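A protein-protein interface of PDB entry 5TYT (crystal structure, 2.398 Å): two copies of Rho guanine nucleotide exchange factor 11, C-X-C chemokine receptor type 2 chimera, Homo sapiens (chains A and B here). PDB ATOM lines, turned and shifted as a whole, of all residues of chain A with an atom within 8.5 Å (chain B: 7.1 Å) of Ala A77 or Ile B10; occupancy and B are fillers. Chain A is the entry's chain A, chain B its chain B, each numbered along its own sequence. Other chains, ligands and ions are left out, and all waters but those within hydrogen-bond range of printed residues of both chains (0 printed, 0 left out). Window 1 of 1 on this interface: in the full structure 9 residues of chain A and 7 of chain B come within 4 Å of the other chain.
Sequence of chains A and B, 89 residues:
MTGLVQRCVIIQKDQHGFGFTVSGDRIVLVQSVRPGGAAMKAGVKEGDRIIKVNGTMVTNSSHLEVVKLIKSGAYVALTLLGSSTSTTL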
ATOM      1  N   ARG A   7      13.021 -23.622 -25.639  1.00  0.00           N
ATOM      2  CA  ARG A   7      14.052 -23.793 -26.659  1.00  0.00           C
ATOM      3  C   ARG A   7      14.734 -22.484 -27.055  1.00  0.00           C
ATOM      4  O   ARG A   7      14.144 -21.421 -26.989  1.00  0.00           O
ATOM      5  CB  ARG A   7      13.462 -24.451 -27.903  1.00  0.00           C
ATOM      6  CG  ARG A   7      13.106 -23.492 -29.032  1.00  0.00           C
ATOM      7  CD  ARG A   7      12.812 -24.250 -30.323  1.00  0.00           C
ATOM      8  NE  ARG A   7      11.406 -24.625 -30.456  1.00  0.00           N
ATOM      9  CZ  ARG A   7      10.545 -24.009 -31.259  1.00  0.00           C
ATOM     10  NH1 ARG A   7      10.959 -22.990 -32.003  1.00  0.00           N
ATOM     11  NH2 ARG A   7       9.272 -24.412 -31.322  1.00  0.00           N
ATOM     12  N   CYS A   8      16.010 -22.567 -27.413  1.00  0.00           N
ATOM     13  CA  CYS A   8      16.760 -21.369 -27.760  1.00  0.00           C
ATOM     14  C   CYS A   8      17.123 -21.304 -29.231  1.00  0.00           C
ATOM     15  O   CYS A   8      17.465 -22.314 -29.846  1.00  0.00           O
ATOM     16  CB  CYS A   8      18.027 -21.269 -26.906  1.00  0.00           C
ATOM     17  SG  CYS A   8      17.815 -21.829 -25.207  1.00  0.00           S
ATOM     18  N   VAL A   9      17.050 -20.103 -29.793  1.00  0.00           N
ATOM     19  CA  VAL A   9      17.388 -19.917 -31.205  1.00  0.00           C
ATOM     20  C   VAL A   9      18.128 -18.626 -31.431  1.00  0.00           C
ATOM     21  O   VAL A   9      17.844 -17.619 -30.790  1.00  0.00           O
ATOM     22  CB  VAL A   9      16.136 -19.928 -32.157  1.00  0.00           C
ATOM     23  CG1 VAL A   9      15.647 -21.343 -32.391  1.00  0.00           C
ATOM     24  CG2 VAL A   9      15.006 -19.031 -31.628  1.00  0.00           C
ATOM     25  N   ILE A  10      19.096 -18.669 -32.337  1.00  0.00           N
ATOM     26  CA  ILE A  10      19.726 -17.458 -32.829  1.00  0.00           C
ATOM     27  C   ILE A  10      19.128 -17.140 -34.179  1.00  0.00           C
ATOM     28  O   ILE A  10      18.955 -18.034 -35.006  1.00  0.00           O
ATOM     29  CB  ILE A  10      21.260 -17.598 -32.974  1.00  0.00           C
ATOM     30  CG1 ILE A  10      21.907 -17.820 -31.609  1.00  0.00           C
ATOM     31  CG2 ILE A  10      21.857 -16.356 -33.657  1.00  0.00           C
ATOM     32  CD1 ILE A  10      22.062 -16.555 -30.796  1.00  0.00           C
ATOM     33  N   ILE A  11      18.800 -15.873 -34.401  1.00  0.00           N
ATOM     34  CA  ILE A  11      18.398 -15.431 -35.734  1.00  0.00           C
ATOM     35  C   ILE A  11      19.362 -14.366 -36.216  1.00  0.00           C
ATOM     36  O   ILE A  11      19.524 -13.346 -35.548  1.00  0.00           O
ATOM     37  CB  ILE A  11      16.951 -14.848 -35.761  1.00  0.00           C
ATOM     38  CG1 ILE A  11      16.014 -15.641 -34.845  1.00  0.00           C
ATOM     39  CG2 ILE A  11      16.430 -14.811 -37.187  1.00  0.00           C
ATOM     40  CD1 ILE A  11      14.538 -15.260 -34.998  1.00  0.00           C
ATOM     41  N   GLN A  12      19.942 -14.565 -37.383  1.00  0.00           N
ATOM     42  CA  GLN A  12      20.757 -13.535 -37.982  1.00  0.00           C
ATOM     43  C   GLN A  12      19.959 -12.717 -38.977  1.00  0.00           C
ATOM     44  O   GLN A  12      19.309 -13.254 -39.816  1.00  0.00           O
ATOM     45  CB  GLN A  12      21.977 -14.128 -38.672  1.00  0.00           C
ATOM     46  CG  GLN A  12      23.141 -14.448 -37.774  1.00  0.00           C
ATOM     47  CD  GLN A  12      24.030 -13.261 -37.506  1.00  0.00           C
ATOM     48  OE1 GLN A  12      23.894 -12.229 -38.107  1.00  0.00           O
ATOM     49  NE2 GLN A  12      24.942 -13.417 -36.589  1.00  0.00           N
ATOM     50  N   PHE A  18      14.632  -9.955 -39.783  1.00  0.00           N
ATOM     51  CA  PHE A  18      14.579 -11.241 -39.087  1.00  0.00           C
ATOM     52  C   PHE A  18      13.589 -12.246 -39.676  1.00  0.00           C
ATOM     53  O   PHE A  18      13.753 -13.458 -39.510  1.00  0.00           O
ATOM     54  CB  PHE A  18      14.253 -11.013 -37.615  1.00  0.00           C
ATOM     55  CG  PHE A  18      15.368 -10.369 -36.842  1.00  0.00           C
ATOM     56  CD1 PHE A  18      16.550 -11.059 -36.592  1.00  0.00           C
ATOM     57  CD2 PHE A  18      15.232  -9.084 -36.346  1.00  0.00           C
ATOM     58  CE1 PHE A  18      17.573 -10.475 -35.867  1.00  0.00           C
ATOM     59  CE2 PHE A  18      16.243  -8.495 -35.618  1.00  0.00           C
ATOM     60  CZ  PHE A  18      17.420  -9.195 -35.382  1.00  0.00           C
ATOM     61  N   ILE A  50       7.728 -15.793 -26.800  1.00  0.00           N
ATOM     62  CA  ILE A  50       9.033 -15.256 -26.497  1.00  0.00           C
ATOM     63  C   ILE A  50       9.193 -15.035 -24.991  1.00  0.00           C
ATOM     64  O   ILE A  50       8.540 -14.170 -24.396  1.00  0.00           O
ATOM     65  CB  ILE A  50       9.271 -13.947 -27.259  1.00  0.00           C
ATOM     66  CG1 ILE A  50       8.982 -14.160 -28.757  1.00  0.00           C
ATOM     67  CG2 ILE A  50      10.689 -13.434 -27.019  1.00  0.00           C
ATOM     68  CD1 ILE A  50       9.470 -13.026 -29.669  1.00  0.00           C
ATOM     69  N   ILE A  51      10.068 -15.840 -24.387  1.00  0.00           N
ATOM     70  CA  ILE A  51      10.375 -15.767 -22.955  1.00  0.00           C
ATOM     71  C   ILE A  51      11.555 -14.811 -22.695  1.00  0.00           C
ATOM     72  O   ILE A  51      11.510 -13.979 -21.793  1.00  0.00           O
ATOM     73  CB  ILE A  51      10.704 -17.174 -22.397  1.00  0.00           C
ATOM     74  CG1 ILE A  51       9.531 -18.120 -22.621  1.00  0.00           C
ATOM     75  CG2 ILE A  51      11.102 -17.114 -20.923  1.00  0.00           C
ATOM     76  CD1 ILE A  51       8.221 -17.524 -22.186  1.00  0.00           C
ATOM     77  N   LYS A  52      12.604 -14.918 -23.502  1.00  0.00           N
ATOM     78  CA  LYS A  52      13.792 -14.079 -23.314  1.00  0.00           C
ATOM     79  C   LYS A  52      14.308 -13.553 -24.641  1.00  0.00           C
ATOM     80  O   LYS A  52      14.252 -14.248 -25.654  1.00  0.00           O
ATOM     81  CB  LYS A  52      14.932 -14.852 -22.606  1.00  0.00           C
ATOM     82  CG  LYS A  52      14.689 -15.205 -21.140  1.00  0.00           C
ATOM     83  CD  LYS A  52      15.808 -16.095 -20.572  1.00  0.00           C
ATOM     84  CE  LYS A  52      17.140 -15.366 -20.536  1.00  0.00           C
ATOM     85  NZ  LYS A  52      18.227 -16.155 -19.882  1.00  0.00           N
ATOM     86  N   VAL A  53      14.836 -12.333 -24.619  1.00  0.00           N
ATOM     87  CA  VAL A  53      15.485 -11.710 -25.779  1.00  0.00           C
ATOM     88  C   VAL A  53      16.887 -11.237 -25.395  1.00  0.00           C
ATOM     89  O   VAL A  53      17.034 -10.372 -24.526  1.00  0.00           O
ATOM     90  CB  VAL A  53      14.677 -10.494 -26.315  1.00  0.00           C
ATOM     91  CG1 VAL A  53      15.393  -9.860 -27.511  1.00  0.00           C
ATOM     92  CG2 VAL A  53      13.249 -10.912 -26.688  1.00  0.00           C
ATOM     93  N   ASN A  54      17.909 -11.783 -26.046  1.00  0.00           N
ATOM     94  CA  ASN A  54      19.284 -11.460 -25.694  1.00  0.00           C
ATOM     95  C   ASN A  54      19.525 -11.517 -24.176  1.00  0.00           C
ATOM     96  O   ASN A  54      20.064 -10.574 -23.586  1.00  0.00           O
ATOM     97  CB  ASN A  54      19.657 -10.077 -26.215  1.00  0.00           C
ATOM     98  CG  ASN A  54      19.435  -9.924 -27.710  1.00  0.00           C
ATOM     99  OD1 ASN A  54      19.554 -10.876 -28.486  1.00  0.00           O
ATOM    100  ND2 ASN A  54      19.105  -8.705 -28.121  1.00  0.00           N
ATOM    101  N   GLY A  55      19.081 -12.600 -23.546  1.00  0.00           N
ATOM    102  CA  GLY A  55      19.300 -12.808 -22.125  1.00  0.00           C
ATOM    103  C   GLY A  55      18.354 -12.109 -21.156  1.00  0.00           C
ATOM    104  O   GLY A  55      18.415 -12.374 -19.963  1.00  0.00           O
ATOM    105  N   THR A  56      17.493 -11.228 -21.660  1.00  0.00           N
ATOM    106  CA  THR A  56      16.561 -10.448 -20.834  1.00  0.00           C
ATOM    107  C   THR A  56      15.149 -11.054 -20.741  1.00  0.00           C
ATOM    108  O   THR A  56      14.504 -11.287 -21.762  1.00  0.00           O
ATOM    109  CB  THR A  56      16.420  -9.021 -21.379  1.00  0.00           C
ATOM    110  OG1 THR A  56      17.702  -8.401 -21.422  1.00  0.00           O
ATOM    111  CG2 THR A  56      15.502  -8.195 -20.494  1.00  0.00           C
ATOM    112  N   VAL A  58      11.540 -11.190 -20.838  1.00  0.00           N
ATOM    113  CA  VAL A  58      10.606 -10.229 -21.415  1.00  0.00           C
ATOM    114  C   VAL A  58       9.160 -10.623 -21.190  1.00  0.00           C
ATOM    115  O   VAL A  58       8.254 -10.004 -21.731  1.00  0.00           O
ATOM    116  CB  VAL A  58      10.841 -10.047 -22.914  1.00  0.00           C
ATOM    117  CG1 VAL A  58      12.121  -9.270 -23.142  1.00  0.00           C
ATOM    118  CG2 VAL A  58      10.876 -11.390 -23.609  1.00  0.00           C
ATOM    119  N   LEU A  69      14.427  -4.449 -27.934  1.00  0.00           N
ATOM    120  CA  LEU A  69      15.402  -5.478 -27.591  1.00  0.00           C
ATOM    121  C   LEU A  69      15.748  -6.366 -28.778  1.00  0.00           C
ATOM    122  O   LEU A  69      16.920  -6.689 -29.006  1.00  0.00           O
ATOM    123  CB  LEU A  69      14.877  -6.341 -26.450  1.00  0.00           C
ATOM    124  CG  LEU A  69      14.883  -5.673 -25.090  1.00  0.00           C
ATOM    125  CD1 LEU A  69      13.970  -6.427 -24.166  1.00  0.00           C
ATOM    126  CD2 LEU A  69      16.290  -5.661 -24.552  1.00  0.00           C
ATOM    127  N   ILE A  70      14.724  -6.769 -29.528  1.00  0.00           N
ATOM    128  CA  ILE A  70      14.935  -7.662 -30.675  1.00  0.00           C
ATOM    129  C   ILE A  70      15.746  -6.976 -31.786  1.00  0.00           C
ATOM    130  O   ILE A  70      16.667  -7.564 -32.361  1.00  0.00           O
ATOM    131  CB  ILE A  70      13.578  -8.173 -31.240  1.00  0.00           C
ATOM    132  CG1 ILE A  70      12.925  -9.122 -30.236  1.00  0.00           C
ATOM    133  CG2 ILE A  70      13.754  -8.845 -32.597  1.00  0.00           C
ATOM    134  CD1 ILE A  70      11.635  -9.759 -30.729  1.00  0.00           C
ATOM    135  N   SER A  72      17.836  -4.610 -31.475  1.00  0.00           N
ATOM    136  CA  SER A  72      19.090  -4.012 -31.001  1.00  0.00           C
ATOM    137  C   SER A  72      20.382  -4.526 -31.684  1.00  0.00           C
ATOM    138  O   SER A  72      21.351  -3.771 -31.829  1.00  0.00           O
ATOM    139  CB  SER A  72      19.218  -4.200 -29.487  1.00  0.00           C
ATOM    140  OG  SER A  72      19.505  -5.539 -29.148  1.00  0.00           O
ATOM    141  N   GLY A  73      20.411  -5.791 -32.093  1.00  0.00           N
ATOM    142  CA  GLY A  73      21.595  -6.325 -32.738  1.00  0.00           C
ATOM    143  C   GLY A  73      21.404  -6.928 -34.122  1.00  0.00           C
ATOM    144  O   GLY A  73      20.281  -7.098 -34.595  1.00  0.00           O
ATOM    145  N   ALA A  74      22.528  -7.261 -34.754  1.00  0.00           N
ATOM    146  CA  ALA A  74      22.582  -7.969 -36.040  1.00  0.00           C
ATOM    147  C   ALA A  74      22.000  -9.370 -35.934  1.00  0.00           C
ATOM    148  O   ALA A  74      21.434  -9.909 -36.884  1.00  0.00           O
ATOM    149  CB  ALA A  74      24.048  -8.040 -36.548  1.00  0.00           C
ATOM    150  N   TYR A  75      22.176  -9.968 -34.767  1.00  0.00           N
ATOM    151  CA  TYR A  75      21.566 -11.243 -34.481  1.00  0.00           C
ATOM    152  C   TYR A  75      20.737 -11.051 -33.222  1.00  0.00           C
ATOM    153  O   TYR A  75      20.963 -10.105 -32.476  1.00  0.00           O
ATOM    154  CB  TYR A  75      22.627 -12.349 -34.302  1.00  0.00           C
ATOM    155  CG  TYR A  75      23.410 -12.284 -32.998  1.00  0.00           C
ATOM    156  CD1 TYR A  75      22.915 -12.869 -31.829  1.00  0.00           C
ATOM    157  CD2 TYR A  75      24.637 -11.635 -32.934  1.00  0.00           C
ATOM    158  CE1 TYR A  75      23.627 -12.806 -30.640  1.00  0.00           C
ATOM    159  CE2 TYR A  75      25.360 -11.575 -31.748  1.00  0.00           C
ATOM    160  CZ  TYR A  75      24.851 -12.162 -30.607  1.00  0.00           C
ATOM    161  OH  TYR A  75      25.553 -12.096 -29.422  1.00  0.00           O
ATOM    162  N   VAL A  76      19.782 -11.940 -32.981  1.00  0.00           N
ATOM    163  CA  VAL A  76      19.042 -11.914 -31.717  1.00  0.00           C
ATOM    164  C   VAL A  76      19.030 -13.320 -31.138  1.00  0.00           C
ATOM    165  O   VAL A  76      18.928 -14.312 -31.895  1.00  0.00           O
ATOM    166  CB  VAL A  76      17.577 -11.391 -31.894  1.00  0.00           C
ATOM    167  CG1 VAL A  76      16.811 -12.258 -32.841  1.00  0.00           C
ATOM    168  CG2 VAL A  76      16.864 -11.303 -30.562  1.00  0.00           C
ATOM    169  N   ALA A  77      19.151 -13.395 -29.813  1.00  0.00           N
ATOM    170  CA  ALA A  77      19.042 -14.645 -29.068  1.00  0.00           C
ATOM    171  C   ALA A  77      17.669 -14.772 -28.405  1.00  0.00           C
ATOM    172  O   ALA A  77      17.337 -13.986 -27.530  1.00  0.00           O
ATOM    173  CB  ALA A  77      20.126 -14.721 -28.018  1.00  0.00           C
ATOM    174  N   LEU A  78      16.888 -15.771 -28.803  1.00  0.00           N
ATOM    175  CA  LEU A  78      15.538 -15.939 -28.280  1.00  0.00           C
ATOM    176  C   LEU A  78      15.422 -17.182 -27.443  1.00  0.00           C
ATOM    177  O   LEU A  78      15.852 -18.254 -27.866  1.00  0.00           O
ATOM    178  CB  LEU A  78      14.512 -16.009 -29.414  1.00  0.00           C
ATOM    179  CG  LEU A  78      14.443 -14.743 -30.248  1.00  0.00           C
ATOM    180  CD1 LEU A  78      13.636 -14.971 -31.526  1.00  0.00           C
ATOM    181  CD2 LEU A  78      13.905 -13.609 -29.413  1.00  0.00           C
ATOM    182  N   THR A  79      14.846 -17.032 -26.255  1.00  0.00           N
ATOM    183  CA  THR A  79      14.343 -18.172 -25.522  1.00  0.00           C
ATOM    184  C   THR A  79      12.834 -18.201 -25.736  1.00  0.00           C
ATOM    185  O   THR A  79      12.108 -17.269 -25.354  1.00  0.00           O
ATOM    186  CB  THR A  79      14.682 -18.115 -24.027  1.00  0.00           C
ATOM    187  OG1 THR A  79      16.103 -18.103 -23.879  1.00  0.00           O
ATOM    188  CG2 THR A  79      14.109 -19.344 -23.294  1.00  0.00           C
ATOM    189  N   LEU A  80      12.409 -19.285 -26.377  1.00  0.00           N
ATOM    190  CA  LEU A  80      11.074 -19.506 -26.901  1.00  0.00           C
ATOM    191  C   LEU A  80      10.368 -20.632 -26.172  1.00  0.00           C
ATOM    192  O   LEU A  80      10.996 -21.620 -25.808  1.00  0.00           O
ATOM    193  CB  LEU A  80      11.133 -19.864 -28.390  1.00  0.00           C
ATOM    194  CG  LEU A  80      11.533 -18.799 -29.403  1.00  0.00           C
ATOM    195  CD1 LEU A  80      11.579 -19.382 -30.807  1.00  0.00           C
ATOM    196  CD2 LEU A  80      10.516 -17.638 -29.325  1.00  0.00           C
ATOM    197  N   CYS B   8      18.367 -25.040 -21.829  1.00  0.00           N
ATOM    198  CA  CYS B   8      19.316 -24.443 -22.740  1.00  0.00           C
ATOM    199  C   CYS B   8      19.443 -22.959 -22.568  1.00  0.00           C
ATOM    200  O   CYS B   8      18.512 -22.298 -22.210  1.00  0.00           O
ATOM    201  CB  CYS B   8      19.006 -24.803 -24.188  1.00  0.00           C
ATOM    202  SG  CYS B   8      17.574 -23.845 -24.939  1.00  0.00           S
ATOM    203  N   VAL B   9      20.631 -22.450 -22.812  1.00  0.00           N
ATOM    204  CA  VAL B   9      20.858 -21.005 -22.760  1.00  0.00           C
ATOM    205  C   VAL B   9      21.805 -20.582 -23.875  1.00  0.00           C
ATOM    206  O   VAL B   9      22.542 -21.392 -24.442  1.00  0.00           O
ATOM    207  CB  VAL B   9      21.480 -20.506 -21.412  1.00  0.00           C
ATOM    208  CG1 VAL B   9      20.605 -20.850 -20.207  1.00  0.00           C
ATOM    209  CG2 VAL B   9      22.891 -21.045 -21.236  1.00  0.00           C
ATOM    210  N   ILE B  10      21.770 -19.296 -24.182  1.00  0.00           N
ATOM    211  CA  ILE B  10      22.705 -18.690 -25.110  1.00  0.00           C
ATOM    212  C   ILE B  10      23.494 -17.611 -24.384  1.00  0.00           C
ATOM    213  O   ILE B  10      22.927 -16.785 -23.676  1.00  0.00           O
ATOM    214  CB  ILE B  10      21.985 -18.085 -26.320  1.00  0.00           C
ATOM    215  CG1 ILE B  10      21.195 -19.173 -27.050  1.00  0.00           C
ATOM    216  CG2 ILE B  10      22.974 -17.418 -27.248  1.00  0.00           C
ATOM    217  CD1 ILE B  10      20.410 -18.682 -28.248  1.00  0.00           C
ATOM    218  N   ILE B  11      24.812 -17.642 -24.523  1.00  0.00           N
ATOM    219  CA  ILE B  11      25.635 -16.594 -23.943  1.00  0.00           C
ATOM    220  C   ILE B  11      26.082 -15.654 -25.044  1.00  0.00           C
ATOM    221  O   ILE B  11      26.536 -16.084 -26.097  1.00  0.00           O
ATOM    222  CB  ILE B  11      26.859 -17.161 -23.208  1.00  0.00           C
ATOM    223  CG1 ILE B  11      26.424 -18.239 -22.218  1.00  0.00           C
ATOM    224  CG2 ILE B  11      27.608 -16.062 -22.477  1.00  0.00           C
ATOM    225  CD1 ILE B  11      27.605 -18.876 -21.466  1.00  0.00           C
ATOM    226  N   GLN B  12      25.906 -14.367 -24.803  1.00  0.00           N
ATOM    227  CA  GLN B  12      26.386 -13.353 -25.713  1.00  0.00           C
ATOM    228  C   GLN B  12      27.726 -12.839 -25.218  1.00  0.00           C
ATOM    229  O   GLN B  12      27.833 -12.354 -24.099  1.00  0.00           O
ATOM    230  CB  GLN B  12      25.379 -12.222 -25.818  1.00  0.00           C
ATOM    231  CG  GLN B  12      24.009 -12.682 -26.245  1.00  0.00           C
ATOM    232  CD  GLN B  12      23.134 -11.538 -26.691  1.00  0.00           C
ATOM    233  OE1 GLN B  12      22.136 -11.741 -27.371  1.00  0.00           O
ATOM    234  NE2 GLN B  12      23.512 -10.321 -26.321  1.00  0.00           N
ATOM    235  N   ALA B  38      28.419 -12.053 -18.793  1.00  0.00           N
ATOM    236  CA  ALA B  38      27.492 -12.543 -19.805  1.00  0.00           C
ATOM    237  C   ALA B  38      26.849 -13.854 -19.380  1.00  0.00           C
ATOM    238  O   ALA B  38      25.628 -13.983 -19.416  1.00  0.00           O
ATOM    239  CB  ALA B  38      28.203 -12.715 -21.128  1.00  0.00           C
ATOM    240  N   ALA B  39      27.673 -14.820 -18.972  1.00  0.00           N
ATOM    241  CA  ALA B  39      27.170 -16.121 -18.533  1.00  0.00           C
ATOM    242  C   ALA B  39      26.167 -15.980 -17.362  1.00  0.00           C
ATOM    243  O   ALA B  39      25.119 -16.631 -17.344  1.00  0.00           O
ATOM    244  CB  ALA B  39      28.341 -17.040 -18.145  1.00  0.00           C
ATOM    245  N   LYS B  41      24.361 -13.497 -16.853  1.00  0.00           N
ATOM    246  CA  LYS B  41      23.240 -12.777 -17.438  1.00  0.00           C
ATOM    247  C   LYS B  41      22.330 -13.712 -18.239  1.00  0.00           C
ATOM    248  O   LYS B  41      21.121 -13.479 -18.342  1.00  0.00           O
ATOM    249  CB  LYS B  41      23.782 -11.632 -18.312  1.00  0.00           C
ATOM    250  CG  LYS B  41      23.017 -11.296 -19.597  1.00  0.00           C
ATOM    251  CD  LYS B  41      23.807 -10.292 -20.453  1.00  0.00           C
ATOM    252  CE  LYS B  41      23.061  -9.914 -21.729  1.00  0.00           C
ATOM    253  NZ  LYS B  41      21.727  -9.281 -21.466  1.00  0.00           N
ATOM    254  N   ALA B  42      22.916 -14.783 -18.774  1.00  0.00           N
ATOM    255  CA  ALA B  42      22.184 -15.746 -19.593  1.00  0.00           C
ATOM    256  C   ALA B  42      21.549 -16.870 -18.767  1.00  0.00           C
ATOM    257  O   ALA B  42      20.753 -17.644 -19.290  1.00  0.00           O
ATOM    258  CB  ALA B  42      23.107 -16.332 -20.651  1.00  0.00           C
ATOM    259  N   GLY B  43      21.904 -16.960 -17.487  1.00  0.00           N
ATOM    260  CA  GLY B  43      21.338 -17.959 -16.595  1.00  0.00           C
ATOM    261  C   GLY B  43      22.263 -19.123 -16.222  1.00  0.00           C
ATOM    262  O   GLY B  43      21.831 -20.116 -15.624  1.00  0.00           O
ATOM    263  N   VAL B  44      23.542 -19.016 -16.573  1.00  0.00           N
ATOM    264  CA  VAL B  44      24.486 -20.081 -16.255  1.00  0.00           C
ATOM    265  C   VAL B  44      24.769 -20.148 -14.738  1.00  0.00           C
ATOM    266  O   VAL B  44      25.043 -19.132 -14.097  1.00  0.00           O
ATOM    267  CB  VAL B  44      25.794 -19.894 -17.039  1.00  0.00           C
ATOM    268  CG1 VAL B  44      26.787 -20.995 -16.708  1.00  0.00           C
ATOM    269  CG2 VAL B  44      25.500 -19.885 -18.525  1.00  0.00           C
ATOM    270  N   TYR B  75      28.745 -15.729 -29.934  1.00  0.00           N
ATOM    271  CA  TYR B  75      27.800 -16.232 -28.944  1.00  0.00           C
ATOM    272  C   TYR B  75      28.005 -17.733 -28.787  1.00  0.00           C
ATOM    273  O   TYR B  75      28.627 -18.363 -29.644  1.00  0.00           O
ATOM    274  CB  TYR B  75      26.361 -15.940 -29.367  1.00  0.00           C
ATOM    275  CG  TYR B  75      25.974 -16.652 -30.647  1.00  0.00           C
ATOM    276  CD1 TYR B  75      25.517 -17.968 -30.623  1.00  0.00           C
ATOM    277  CD2 TYR B  75      26.084 -16.017 -31.883  1.00  0.00           C
ATOM    278  CE1 TYR B  75      25.178 -18.634 -31.791  1.00  0.00           C
ATOM    279  CE2 TYR B  75      25.733 -16.675 -33.063  1.00  0.00           C
ATOM    280  CZ  TYR B  75      25.282 -17.986 -33.007  1.00  0.00           C
ATOM    281  OH  TYR B  75      24.924 -18.649 -34.164  1.00  0.00           O
ATOM    282  N   VAL B  76      27.472 -18.328 -27.725  1.00  0.00           N
ATOM    283  CA  VAL B  76      27.494 -19.790 -27.659  1.00  0.00           C
ATOM    284  C   VAL B  76      26.177 -20.362 -27.137  1.00  0.00           C
ATOM    285  O   VAL B  76      25.635 -19.931 -26.103  1.00  0.00           O
ATOM    286  CB  VAL B  76      28.679 -20.322 -26.799  1.00  0.00           C
ATOM    287  CG1 VAL B  76      28.580 -19.847 -25.360  1.00  0.00           C
ATOM    288  CG2 VAL B  76      28.760 -21.847 -26.876  1.00  0.00           C
ATOM    289  N   ALA B  77      25.645 -21.321 -27.892  1.00  0.00           N
ATOM    290  CA  ALA B  77      24.472 -22.065 -27.457  1.00  0.00           C
ATOM    291  C   ALA B  77      24.930 -23.263 -26.646  1.00  0.00           C
ATOM    292  O   ALA B  77      25.663 -24.112 -27.154  1.00  0.00           O
ATOM    293  CB  ALA B  77      23.624 -22.513 -28.649  1.00  0.00           C
ATOM    294  N   LEU B  78      24.518 -23.313 -25.382  1.00  0.00           N
ATOM    295  CA  LEU B  78      24.843 -24.439 -24.528  1.00  0.00           C
ATOM    296  C   LEU B  78      23.588 -25.157 -24.079  1.00  0.00           C
ATOM    297  O   LEU B  78      22.546 -24.522 -23.824  1.00  0.00           O
ATOM    298  CB  LEU B  78      25.635 -23.994 -23.288  1.00  0.00           C
ATOM    299  CG  LEU B  78      26.985 -23.271 -23.373  1.00  0.00           C
ATOM    300  CD1 LEU B  78      27.260 -22.602 -22.029  1.00  0.00           C
ATOM    301  CD2 LEU B  78      28.146 -24.225 -23.729  1.00  0.00           C
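Cys A8 touches Val B9, but with the chains exchanged Val A9 does not touch Cys B8 (6.2 Å).
Cys A8 touches Ile B10, but with the chains exchanged Ile A10 does not touch Cys B8 (9.2 Å).
Val A9 touches Ile B10, but with the chains exchanged Ile A10 does not touch Val B9 (8.0 Å).
Ala A77 touches Ile B10, but with the chains exchanged Ile A10 does not touch Ala B77 (5.8 Å).
Of the 15 pairs that touch across the chains among the printed residues, 3 have their exchanged pair printed and touching as well.
The side-chain sulfur (SG) of Cys A8 is disulfide-bonded to the side-chain sulfur (SG) of Cys B8 (2.0 Å).
The side-chain sulfur (SG) of Cys A8 lies within hydrogen-bond range of the backbone NH (N) of Val B9, 3.7 Å away.
The side-chain amino group (NZ) of Lys A52 sits at hydrogen-bond distance from the backbone carbonyl oxygen (O) of Ala B42 (3.0 Å).
The side-chain amide oxygen of Asn A54 sits close to the side-chain amide oxygen of Gln B12 (2.9 Å).
The backbone carbonyl oxygen (O) of Asn A54 sits at hydrogen-bond distance from the side-chain amino group (NZ) of Lys B41, at 3.0 Å.
The backbone carbonyl oxygen (O) of Lys B41 lies close to the backbone carbonyl oxygen (O) of Gly A55, 3.3 Å away.
Of the printed residues of chain B, Arg A7 touches Cys B8 (3.8 Å).
Of the printed residues of chain B, Lys A52 touches Ala B42.
Of the printed residues of chain B, Asn A54 touches Gln B12 and Lys B41.
Of the printed residues of chain B, Gly A55 touches Lys B41.
Ala A77 touches two residues of chain B.
Thr A79 touches none of the printed residues of chain B.
Of chain A, only Cys A8 (3.7 Å) comes within 4 Å of Val B9.
Ile B10 touches four residues of chain A.
Of the printed residues of chain A, Gln B12 touches Asn A54, Tyr A75 and Ala A77.
The nearest residue of chain B that does not touch Ala A77 is Tyr B75 (6.5 Å).
The nearest printed residue of chain A that does not touch Gln B12 is Gly A55 (5.0 Å).
Of the 26 printed residues of chain A, 9 touch a printed residue of chain B.
Hydrophobic or aromatic side chains of chain A that line the printed part of chain B: Ile A10, Tyr A75 and Ala A77.
Along chain B the printed residues that touch a printed residue of chain A span positions 8 to 75.
Among the printed residues, 15 pairs touch across the chains.
Arg A7 touches Cys B8.
Cys A8 touches Ile B10 (CB to CD1, 3.8 Å).
Val A9 touches Ile B10.
Ile B10 touches Ile A10 (CD1 to CD1, 3.7 Å).
CG1 of Ile A10 touches CE1 of Tyr B75, 3.4 Å away.
OH of Tyr A75 touches CG of Gln B12 (3.6 Å).
OH of Tyr A75 touches CB of Tyr B75, 3.9 Å away.
Ala A77 touches Ile B10.
Ala A77 touches Gln B12.
The backbone NH (N) of Leu A80 is in hydrogen-bond range of the backbone carbonyl oxygen (O) of Arg A7, 2.8 Å away.
The backbone NH of Leu A78 is in hydrogen-bond range of the backbone carbonyl oxygen of Val A9.
O of Lys A52 is in hydrogen-bond range of N of Thr A79, at 2.9 Å.
The backbone carbonyl oxygen (O) of Leu A69 lies within hydrogen-bond range of the side-chain amide nitrogen (ND2) of Asn A54 (3.1 Å).
ND2 of Asn A54 is in hydrogen-bond range of OG of Ser A72, 3.4 Å away.
The backbone NH of Asn A54 sits at hydrogen-bond distance from the backbone carbonyl oxygen of Ala A77 (2.7 Å).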
